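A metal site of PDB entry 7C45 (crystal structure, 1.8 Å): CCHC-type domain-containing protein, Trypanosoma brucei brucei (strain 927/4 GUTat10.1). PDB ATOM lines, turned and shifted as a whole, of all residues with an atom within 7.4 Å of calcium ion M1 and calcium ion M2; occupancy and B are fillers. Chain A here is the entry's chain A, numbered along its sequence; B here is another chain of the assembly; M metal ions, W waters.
Calcium ion M1 is bound by OD2 of Asp 41 (2.2 Å), OP1 of U 10 of chain B (2.2 Å), OE2 of Glu 43 (2.3 Å), OD2 of Asp 191 (2.4 Å), water W5 (2.5 Å) and water W4 (2.9 Å). Calcium ion M1 has six donor atoms within binding distance. Slightly farther from calcium ion M1 lies OD1 of Asp 41 (3.1 Å).
The backbone carbonyl oxygen of Asp 41 lies within hydrogen-bond range of the backbone NH of Gln 61, at 2.9 Å. OP1 of U 9 of chain B sits at hydrogen-bond distance from N of Met 144 (3.3 Å). N of Glu 43 is in hydrogen-bond range of OE1 of Gln 61, 3.3 Å away.
Within 4 Å of calcium ion M1: Asp 41, Glu 43, Asp 191 and U 10 of chain B. The nearest printed residue that does not touch calcium ion M1 is Gln 61 (4.2 Å).
O3' of U 9 of chain B is bound to calcium ion M2. Calcium ion M2 is bound by water W2, 2.4 Å away. Calcium ion M2 is bound by the side-chain carboxylate (OD1) of Asp 41 (2.4 Å). Calcium ion M2 is bound by water W1, 2.4 Å away. OP1 of U 10 of chain B binds calcium ion M2 (2.5 Å). Water W3 is bound to calcium ion M2 (2.5 Å).
Of the 23 residues printed, 3 come within 4 Å of calcium ion M2.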
ATOM      1  N   LEU A  40     -12.057   9.716 -23.611  1.00  0.00           N
ATOM      2  CA  LEU A  40     -11.683   9.691 -25.021  1.00  0.00           C
ATOM      3  C   LEU A  40     -10.249   9.225 -25.208  1.00  0.00           C
ATOM      4  O   LEU A  40      -9.396   9.416 -24.336  1.00  0.00           O
ATOM      5  CB  LEU A  40     -11.817  11.049 -25.661  1.00  0.00           C
ATOM      6  CG  LEU A  40     -13.243  11.550 -25.846  1.00  0.00           C
ATOM      7  CD1 LEU A  40     -13.214  12.997 -26.281  1.00  0.00           C
ATOM      8  CD2 LEU A  40     -13.990  10.713 -26.877  1.00  0.00           C
ATOM      9  N   ASP A  41      -9.995   8.646 -26.379  1.00  0.00           N
ATOM     10  CA  ASP A  41      -8.692   8.148 -26.768  1.00  0.00           C
ATOM     11  C   ASP A  41      -8.692   8.105 -28.294  1.00  0.00           C
ATOM     12  O   ASP A  41      -9.740   8.098 -28.926  1.00  0.00           O
ATOM     13  CB  ASP A  41      -8.456   6.778 -26.138  1.00  0.00           C
ATOM     14  CG  ASP A  41      -7.054   6.256 -26.316  1.00  0.00           C
ATOM     15  OD1 ASP A  41      -6.131   7.026 -26.593  1.00  0.00           O
ATOM     16  OD2 ASP A  41      -6.895   5.044 -26.149  1.00  0.00           O
ATOM     17  N   ILE A  42      -7.491   8.106 -28.873  1.00  0.00           N
ATOM     18  CA  ILE A  42      -7.374   8.028 -30.337  1.00  0.00           C
ATOM     19  C   ILE A  42      -6.287   7.044 -30.688  1.00  0.00           C
ATOM     20  O   ILE A  42      -5.204   7.053 -30.092  1.00  0.00           O
ATOM     21  CB  ILE A  42      -7.064   9.415 -30.965  1.00  0.00           C
ATOM     22  CG1 ILE A  42      -8.194  10.411 -30.669  1.00  0.00           C
ATOM     23  CG2 ILE A  42      -6.845   9.280 -32.449  1.00  0.00           C
ATOM     24  CD1 ILE A  42      -7.881  11.817 -31.176  1.00  0.00           C
ATOM     25  N   GLU A  43      -6.558   6.175 -31.683  1.00  0.00           N
ATOM     26  CA  GLU A  43      -5.523   5.381 -32.333  1.00  0.00           C
ATOM     27  C   GLU A  43      -5.297   5.901 -33.748  1.00  0.00           C
ATOM     28  O   GLU A  43      -6.246   6.077 -34.515  1.00  0.00           O
ATOM     29  CB  GLU A  43      -5.884   3.901 -32.402  1.00  0.00           C
ATOM     30  CG  GLU A  43      -6.162   3.205 -31.049  1.00  0.00           C
ATOM     31  CD  GLU A  43      -5.114   3.486 -29.980  1.00  0.00           C
ATOM     32  OE1 GLU A  43      -3.919   3.338 -30.295  1.00  0.00           O
ATOM     33  OE2 GLU A  43      -5.494   3.819 -28.816  1.00  0.00           O
ATOM     34  N   LEU A  54       0.395  12.879 -34.393  1.00  0.00           N
ATOM     35  CA  LEU A  54      -0.218  11.586 -34.700  1.00  0.00           C
ATOM     36  C   LEU A  54      -0.366  11.451 -36.209  1.00  0.00           C
ATOM     37  O   LEU A  54      -0.598  12.430 -36.912  1.00  0.00           O
ATOM     38  CB  LEU A  54      -1.592  11.464 -34.046  1.00  0.00           C
ATOM     39  CG  LEU A  54      -1.636  11.349 -32.520  1.00  0.00           C
ATOM     40  CD1 LEU A  54      -3.023  10.993 -32.104  1.00  0.00           C
ATOM     41  CD2 LEU A  54      -0.648  10.333 -31.976  1.00  0.00           C
ATOM     42  N   GLN A  61     -11.967   6.470 -29.663  1.00  0.00           N
ATOM     43  CA  GLN A  61     -12.610   5.583 -28.694  1.00  0.00           C
ATOM     44  C   GLN A  61     -13.296   6.414 -27.619  1.00  0.00           C
ATOM     45  O   GLN A  61     -12.786   7.464 -27.227  1.00  0.00           O
ATOM     46  CB  GLN A  61     -11.605   4.620 -28.088  1.00  0.00           C
ATOM     47  CG  GLN A  61     -10.840   3.833 -29.157  1.00  0.00           C
ATOM     48  CD  GLN A  61      -9.520   4.469 -29.504  1.00  0.00           C
ATOM     49  OE1 GLN A  61      -9.441   5.337 -30.386  1.00  0.00           O
ATOM     50  NE2 GLN A  61      -8.480   4.065 -28.825  1.00  0.00           N
ATOM     51  N   PHE A 100      -9.275  12.706 -20.756  1.00  0.00           N
ATOM     52  CA  PHE A 100      -8.157  12.217 -21.555  1.00  0.00           C
ATOM     53  C   PHE A 100      -7.084  11.679 -20.629  1.00  0.00           C
ATOM     54  O   PHE A 100      -7.083  11.974 -19.438  1.00  0.00           O
ATOM     55  CB  PHE A 100      -7.526  13.322 -22.418  1.00  0.00           C
ATOM     56  CG  PHE A 100      -8.336  13.703 -23.628  1.00  0.00           C
ATOM     57  CD1 PHE A 100      -9.342  14.651 -23.530  1.00  0.00           C
ATOM     58  CD2 PHE A 100      -8.079  13.132 -24.859  1.00  0.00           C
ATOM     59  CE1 PHE A 100     -10.086  15.009 -24.642  1.00  0.00           C
ATOM     60  CE2 PHE A 100      -8.804  13.498 -25.979  1.00  0.00           C
ATOM     61  CZ  PHE A 100      -9.816  14.433 -25.872  1.00  0.00           C
ATOM     62  N   PHE A 101      -6.158  10.920 -21.200  1.00  0.00           N
ATOM     63  CA  PHE A 101      -4.896  10.585 -20.531  1.00  0.00           C
ATOM     64  C   PHE A 101      -3.780  11.005 -21.497  1.00  0.00           C
ATOM     65  O   PHE A 101      -3.480  10.304 -22.480  1.00  0.00           O
ATOM     66  CB  PHE A 101      -4.798   9.110 -20.174  1.00  0.00           C
ATOM     67  CG  PHE A 101      -3.635   8.802 -19.263  1.00  0.00           C
ATOM     68  CD1 PHE A 101      -3.785   8.926 -17.893  1.00  0.00           C
ATOM     69  CD2 PHE A 101      -2.398   8.433 -19.761  1.00  0.00           C
ATOM     70  CE1 PHE A 101      -2.734   8.667 -17.035  1.00  0.00           C
ATOM     71  CE2 PHE A 101      -1.340   8.186 -18.922  1.00  0.00           C
ATOM     72  CZ  PHE A 101      -1.508   8.303 -17.554  1.00  0.00           C
ATOM     73  N   ASP A 102      -3.189  12.170 -21.200  1.00  0.00           N
ATOM     74  CA  ASP A 102      -2.342  12.939 -22.097  1.00  0.00           C
ATOM     75  C   ASP A 102      -3.128  13.349 -23.335  1.00  0.00           C
ATOM     76  O   ASP A 102      -3.189  12.599 -24.312  1.00  0.00           O
ATOM     77  CB  ASP A 102      -1.067  12.169 -22.504  1.00  0.00           C
ATOM     78  CG  ASP A 102      -0.038  13.088 -23.206  1.00  0.00           C
ATOM     79  OD1 ASP A 102      -0.413  14.226 -23.523  1.00  0.00           O
ATOM     80  OD2 ASP A 102       1.106  12.675 -23.431  1.00  0.00           O
ATOM     81  N   CYS A 103      -3.693  14.559 -23.310  1.00  0.00           N
ATOM     82  CA  CYS A 103      -4.548  15.048 -24.385  1.00  0.00           C
ATOM     83  C   CYS A 103      -3.767  15.689 -25.527  1.00  0.00           C
ATOM     84  O   CYS A 103      -4.367  16.047 -26.545  1.00  0.00           O
ATOM     85  CB  CYS A 103      -5.542  16.089 -23.865  1.00  0.00           C
ATOM     86  SG  CYS A 103      -4.833  17.642 -23.283  1.00  0.00           S
ATOM     87  N   ASP A 106      -3.639  14.041 -29.012  1.00  0.00           N
ATOM     88  CA  ASP A 106      -5.034  13.798 -29.402  1.00  0.00           C
ATOM     89  C   ASP A 106      -5.696  15.082 -29.850  1.00  0.00           C
ATOM     90  O   ASP A 106      -6.367  15.117 -30.900  1.00  0.00           O
ATOM     91  CB  ASP A 106      -5.814  13.224 -28.221  1.00  0.00           C
ATOM     92  CG  ASP A 106      -5.415  11.793 -27.906  1.00  0.00           C
ATOM     93  OD1 ASP A 106      -4.685  11.191 -28.700  1.00  0.00           O
ATOM     94  OD2 ASP A 106      -5.883  11.284 -26.867  1.00  0.00           O
ATOM     95  N   MET A 144       0.182   5.229 -18.322  1.00  0.00           N
ATOM     96  CA  MET A 144      -1.094   4.694 -17.842  1.00  0.00           C
ATOM     97  C   MET A 144      -0.907   3.551 -16.849  1.00  0.00           C
ATOM     98  O   MET A 144      -1.636   3.451 -15.862  1.00  0.00           O
ATOM     99  CB  MET A 144      -1.913   4.228 -19.047  1.00  0.00           C
ATOM    100  CG  MET A 144      -3.191   3.521 -18.735  1.00  0.00           C
ATOM    101  SD  MET A 144      -4.427   4.566 -17.957  1.00  0.00           S
ATOM    102  CE  MET A 144      -5.104   5.387 -19.403  1.00  0.00           C
ATOM    103  N   MET A 167       3.558  -2.535 -33.434  1.00  0.00           N
ATOM    104  CA  MET A 167       3.528  -1.095 -33.162  1.00  0.00           C
ATOM    105  C   MET A 167       4.900  -0.558 -32.769  1.00  0.00           C
ATOM    106  O   MET A 167       5.506   0.231 -33.488  1.00  0.00           O
ATOM    107  CB  MET A 167       2.516  -0.795 -32.068  1.00  0.00           C
ATOM    108  CG  MET A 167       2.176   0.654 -31.895  1.00  0.00           C
ATOM    109  SD  MET A 167       0.393   0.778 -31.817  1.00  0.00           S
ATOM    110  CE  MET A 167       0.147   2.176 -30.750  1.00  0.00           C
ATOM    111  N   TRP A 175      -2.666   0.526 -37.781  1.00  0.00           N
ATOM    112  CA  TRP A 175      -4.098   0.754 -37.610  1.00  0.00           C
ATOM    113  C   TRP A 175      -4.821   1.001 -38.930  1.00  0.00           C
ATOM    114  O   TRP A 175      -5.996   1.401 -38.908  1.00  0.00           O
ATOM    115  CB  TRP A 175      -4.315   1.920 -36.647  1.00  0.00           C
ATOM    116  CG  TRP A 175      -3.876   1.582 -35.263  1.00  0.00           C
ATOM    117  CD1 TRP A 175      -2.705   1.930 -34.655  1.00  0.00           C
ATOM    118  CD2 TRP A 175      -4.583   0.776 -34.311  1.00  0.00           C
ATOM    119  NE1 TRP A 175      -2.651   1.419 -33.385  1.00  0.00           N
ATOM    120  CE2 TRP A 175      -3.783   0.692 -33.148  1.00  0.00           C
ATOM    121  CE3 TRP A 175      -5.833   0.127 -34.329  1.00  0.00           C
ATOM    122  CZ2 TRP A 175      -4.183  -0.002 -32.019  1.00  0.00           C
ATOM    123  CZ3 TRP A 175      -6.220  -0.594 -33.218  1.00  0.00           C
ATOM    124  CH2 TRP A 175      -5.403  -0.640 -32.064  1.00  0.00           C
ATOM    125  N   TYR A 187      -7.481  -4.105 -27.760  1.00  0.00           N
ATOM    126  CA  TYR A 187      -6.364  -3.223 -27.448  1.00  0.00           C
ATOM    127  C   TYR A 187      -6.804  -1.772 -27.495  1.00  0.00           C
ATOM    128  O   TYR A 187      -6.607  -1.033 -26.535  1.00  0.00           O
ATOM    129  CB  TYR A 187      -5.212  -3.469 -28.408  1.00  0.00           C
ATOM    130  CG  TYR A 187      -3.999  -2.643 -28.066  1.00  0.00           C
ATOM    131  CD1 TYR A 187      -3.852  -1.358 -28.577  1.00  0.00           C
ATOM    132  CD2 TYR A 187      -3.000  -3.141 -27.228  1.00  0.00           C
ATOM    133  CE1 TYR A 187      -2.749  -0.601 -28.264  1.00  0.00           C
ATOM    134  CE2 TYR A 187      -1.896  -2.383 -26.915  1.00  0.00           C
ATOM    135  CZ  TYR A 187      -1.777  -1.110 -27.439  1.00  0.00           C
ATOM    136  OH  TYR A 187      -0.679  -0.334 -27.147  1.00  0.00           O
ATOM    137  N   ALA A 188      -7.451  -1.362 -28.599  1.00  0.00           N
ATOM    138  CA  ALA A 188      -7.929   0.005 -28.690  1.00  0.00           C
ATOM    139  C   ALA A 188      -8.941   0.336 -27.617  1.00  0.00           C
ATOM    140  O   ALA A 188      -9.064   1.498 -27.217  1.00  0.00           O
ATOM    141  CB  ALA A 188      -8.541   0.261 -30.079  1.00  0.00           C
ATOM    142  N   ALA A 189      -9.706  -0.650 -27.140  1.00  0.00           N
ATOM    143  CA  ALA A 189     -10.758  -0.354 -26.180  1.00  0.00           C
ATOM    144  C   ALA A 189     -10.242  -0.118 -24.769  1.00  0.00           C
ATOM    145  O   ALA A 189     -10.945   0.496 -23.963  1.00  0.00           O
ATOM    146  CB  ALA A 189     -11.782  -1.491 -26.127  1.00  0.00           C
ATOM    147  N   GLY A 190      -9.022  -0.567 -24.454  1.00  0.00           N
ATOM    148  CA  GLY A 190      -8.615  -0.668 -23.066  1.00  0.00           C
ATOM    149  C   GLY A 190      -8.472   0.683 -22.374  1.00  0.00           C
ATOM    150  O   GLY A 190      -8.915   0.859 -21.244  1.00  0.00           O
ATOM    151  N   ASP A 191      -7.834   1.650 -23.043  1.00  0.00           N
ATOM    152  CA  ASP A 191      -7.478   2.873 -22.328  1.00  0.00           C
ATOM    153  C   ASP A 191      -8.695   3.639 -21.825  1.00  0.00           C
ATOM    154  O   ASP A 191      -8.642   4.198 -20.724  1.00  0.00           O
ATOM    155  CB  ASP A 191      -6.618   3.789 -23.196  1.00  0.00           C
ATOM    156  CG  ASP A 191      -5.200   3.298 -23.333  1.00  0.00           C
ATOM    157  OD1 ASP A 191      -4.769   2.449 -22.534  1.00  0.00           O
ATOM    158  OD2 ASP A 191      -4.516   3.761 -24.261  1.00  0.00           O
ATOM    159  N   VAL A 192      -9.779   3.727 -22.613  1.00  0.00           N
ATOM    160  CA  VAL A 192     -10.881   4.569 -22.161  1.00  0.00           C
ATOM    161  C   VAL A 192     -11.598   3.946 -20.972  1.00  0.00           C
ATOM    162  O   VAL A 192     -12.130   4.663 -20.132  1.00  0.00           O
ATOM    163  CB  VAL A 192     -11.883   4.898 -23.287  1.00  0.00           C
ATOM    164  CG1 VAL A 192     -11.296   5.969 -24.235  1.00  0.00           C
ATOM    165  CG2 VAL A 192     -12.345   3.620 -24.022  1.00  0.00           C
ATOM    166  N   ILE A 195      -9.444   5.138 -18.236  1.00  0.00           N
ATOM    167  CA  ILE A 195      -9.666   6.552 -18.001  1.00  0.00           C
ATOM    168  C   ILE A 195     -10.936   6.774 -17.192  1.00  0.00           C
ATOM    169  O   ILE A 195     -10.954   7.566 -16.243  1.00  0.00           O
ATOM    170  CB  ILE A 195      -9.719   7.309 -19.336  1.00  0.00           C
ATOM    171  CG1 ILE A 195      -8.318   7.304 -19.945  1.00  0.00           C
ATOM    172  CG2 ILE A 195     -10.202   8.726 -19.106  1.00  0.00           C
ATOM    173  CD1 ILE A 195      -8.236   7.793 -21.433  1.00  0.00           C
ATOM    174  P     U B   9       1.742   7.007 -22.164  1.00  0.00           P
ATOM    175  OP1   U B   9       0.634   6.486 -21.316  1.00  0.00           O
ATOM    176  OP2   U B   9       2.874   6.127 -22.532  1.00  0.00           O
ATOM    177  O5'   U B   9       1.197   7.694 -23.484  1.00  0.00           O
ATOM    178  C5'   U B   9      -0.104   8.263 -23.568  1.00  0.00           C
ATOM    179  C4'   U B   9      -0.394   8.935 -24.894  1.00  0.00           C
ATOM    180  O4'   U B   9       0.645   9.866 -25.263  1.00  0.00           O
ATOM    181  C3'   U B   9      -0.527   8.044 -26.116  1.00  0.00           C
ATOM    182  O3'   U B   9      -1.765   7.375 -26.182  1.00  0.00           O
ATOM    183  C2'   U B   9      -0.302   9.011 -27.268  1.00  0.00           C
ATOM    184  O2'   U B   9      -1.456   9.791 -27.542  1.00  0.00           O
ATOM    185  C1'   U B   9       0.763   9.931 -26.670  1.00  0.00           C
ATOM    186  N1    U B   9       2.117   9.519 -27.055  1.00  0.00           N
ATOM    187  C2    U B   9       2.560   9.799 -28.344  1.00  0.00           C
ATOM    188  O2    U B   9       1.887  10.375 -29.183  1.00  0.00           O
ATOM    189  N3    U B   9       3.829   9.390 -28.648  1.00  0.00           N
ATOM    190  C4    U B   9       4.698   8.731 -27.800  1.00  0.00           C
ATOM    191  O4    U B   9       5.809   8.414 -28.210  1.00  0.00           O
ATOM    192  C5    U B   9       4.172   8.462 -26.489  1.00  0.00           C
ATOM    193  C6    U B   9       2.931   8.852 -26.162  1.00  0.00           C
ATOM    194  P     U B  10      -1.842   5.895 -26.766  1.00  0.00           P
ATOM    195  OP1   U B  10      -3.278   5.560 -26.767  1.00  0.00           O
ATOM    196  OP2   U B  10      -0.859   5.015 -26.064  1.00  0.00           O
ATOM    197  O5'   U B  10      -1.341   6.056 -28.279  1.00  0.00           O
ATOM    198  C5'   U B  10      -2.191   6.640 -29.244  1.00  0.00           C
ATOM    199  C4'   U B  10      -1.521   6.727 -30.598  1.00  0.00           C
ATOM    200  O4'   U B  10      -0.214   7.311 -30.434  1.00  0.00           O
ATOM    201  C3'   U B  10      -1.242   5.407 -31.292  1.00  0.00           C
ATOM    202  O3'   U B  10      -2.370   4.920 -31.984  1.00  0.00           O
ATOM    203  C2'   U B  10      -0.099   5.754 -32.224  1.00  0.00           C
ATOM    204  O2'   U B  10      -0.600   6.403 -33.378  1.00  0.00           O
ATOM    205  C1'   U B  10       0.676   6.775 -31.384  1.00  0.00           C
ATOM    206  N1    U B  10       1.818   6.167 -30.661  1.00  0.00           N
ATOM    207  C2    U B  10       2.953   5.992 -31.404  1.00  0.00           C
ATOM    208  O2    U B  10       3.010   6.293 -32.589  1.00  0.00           O
ATOM    209  N3    U B  10       3.998   5.439 -30.711  1.00  0.00           N
ATOM    210  C4    U B  10       4.009   5.076 -29.388  1.00  0.00           C
ATOM    211  O4    U B  10       5.025   4.586 -28.910  1.00  0.00           O
ATOM    212  C5    U B  10       2.781   5.298 -28.675  1.00  0.00           C
ATOM    213  C6    U B  10       1.749   5.836 -29.326  1.00  0.00           C
HETATM  214 CA    CA M   1      -4.961   4.107 -26.610  1.00  0.00          CA
HETATM  215 CA    CA M   2      -3.943   7.808 -26.016  1.00  0.00          CA
HETATM  216  O   HOH W   1      -3.924   7.661 -23.581  1.00  0.00           O
HETATM  217  O   HOH W   2      -4.176   8.835 -28.157  1.00  0.00           O
HETATM  218  O   HOH W   3      -4.337  10.133 -25.262  1.00  0.00           O
HETATM  219  O   HOH W   4      -6.231   1.683 -25.754  1.00  0.00           O
HETATM  220  O   HOH W   5      -3.484   2.121 -26.846  1.00  0.00           O
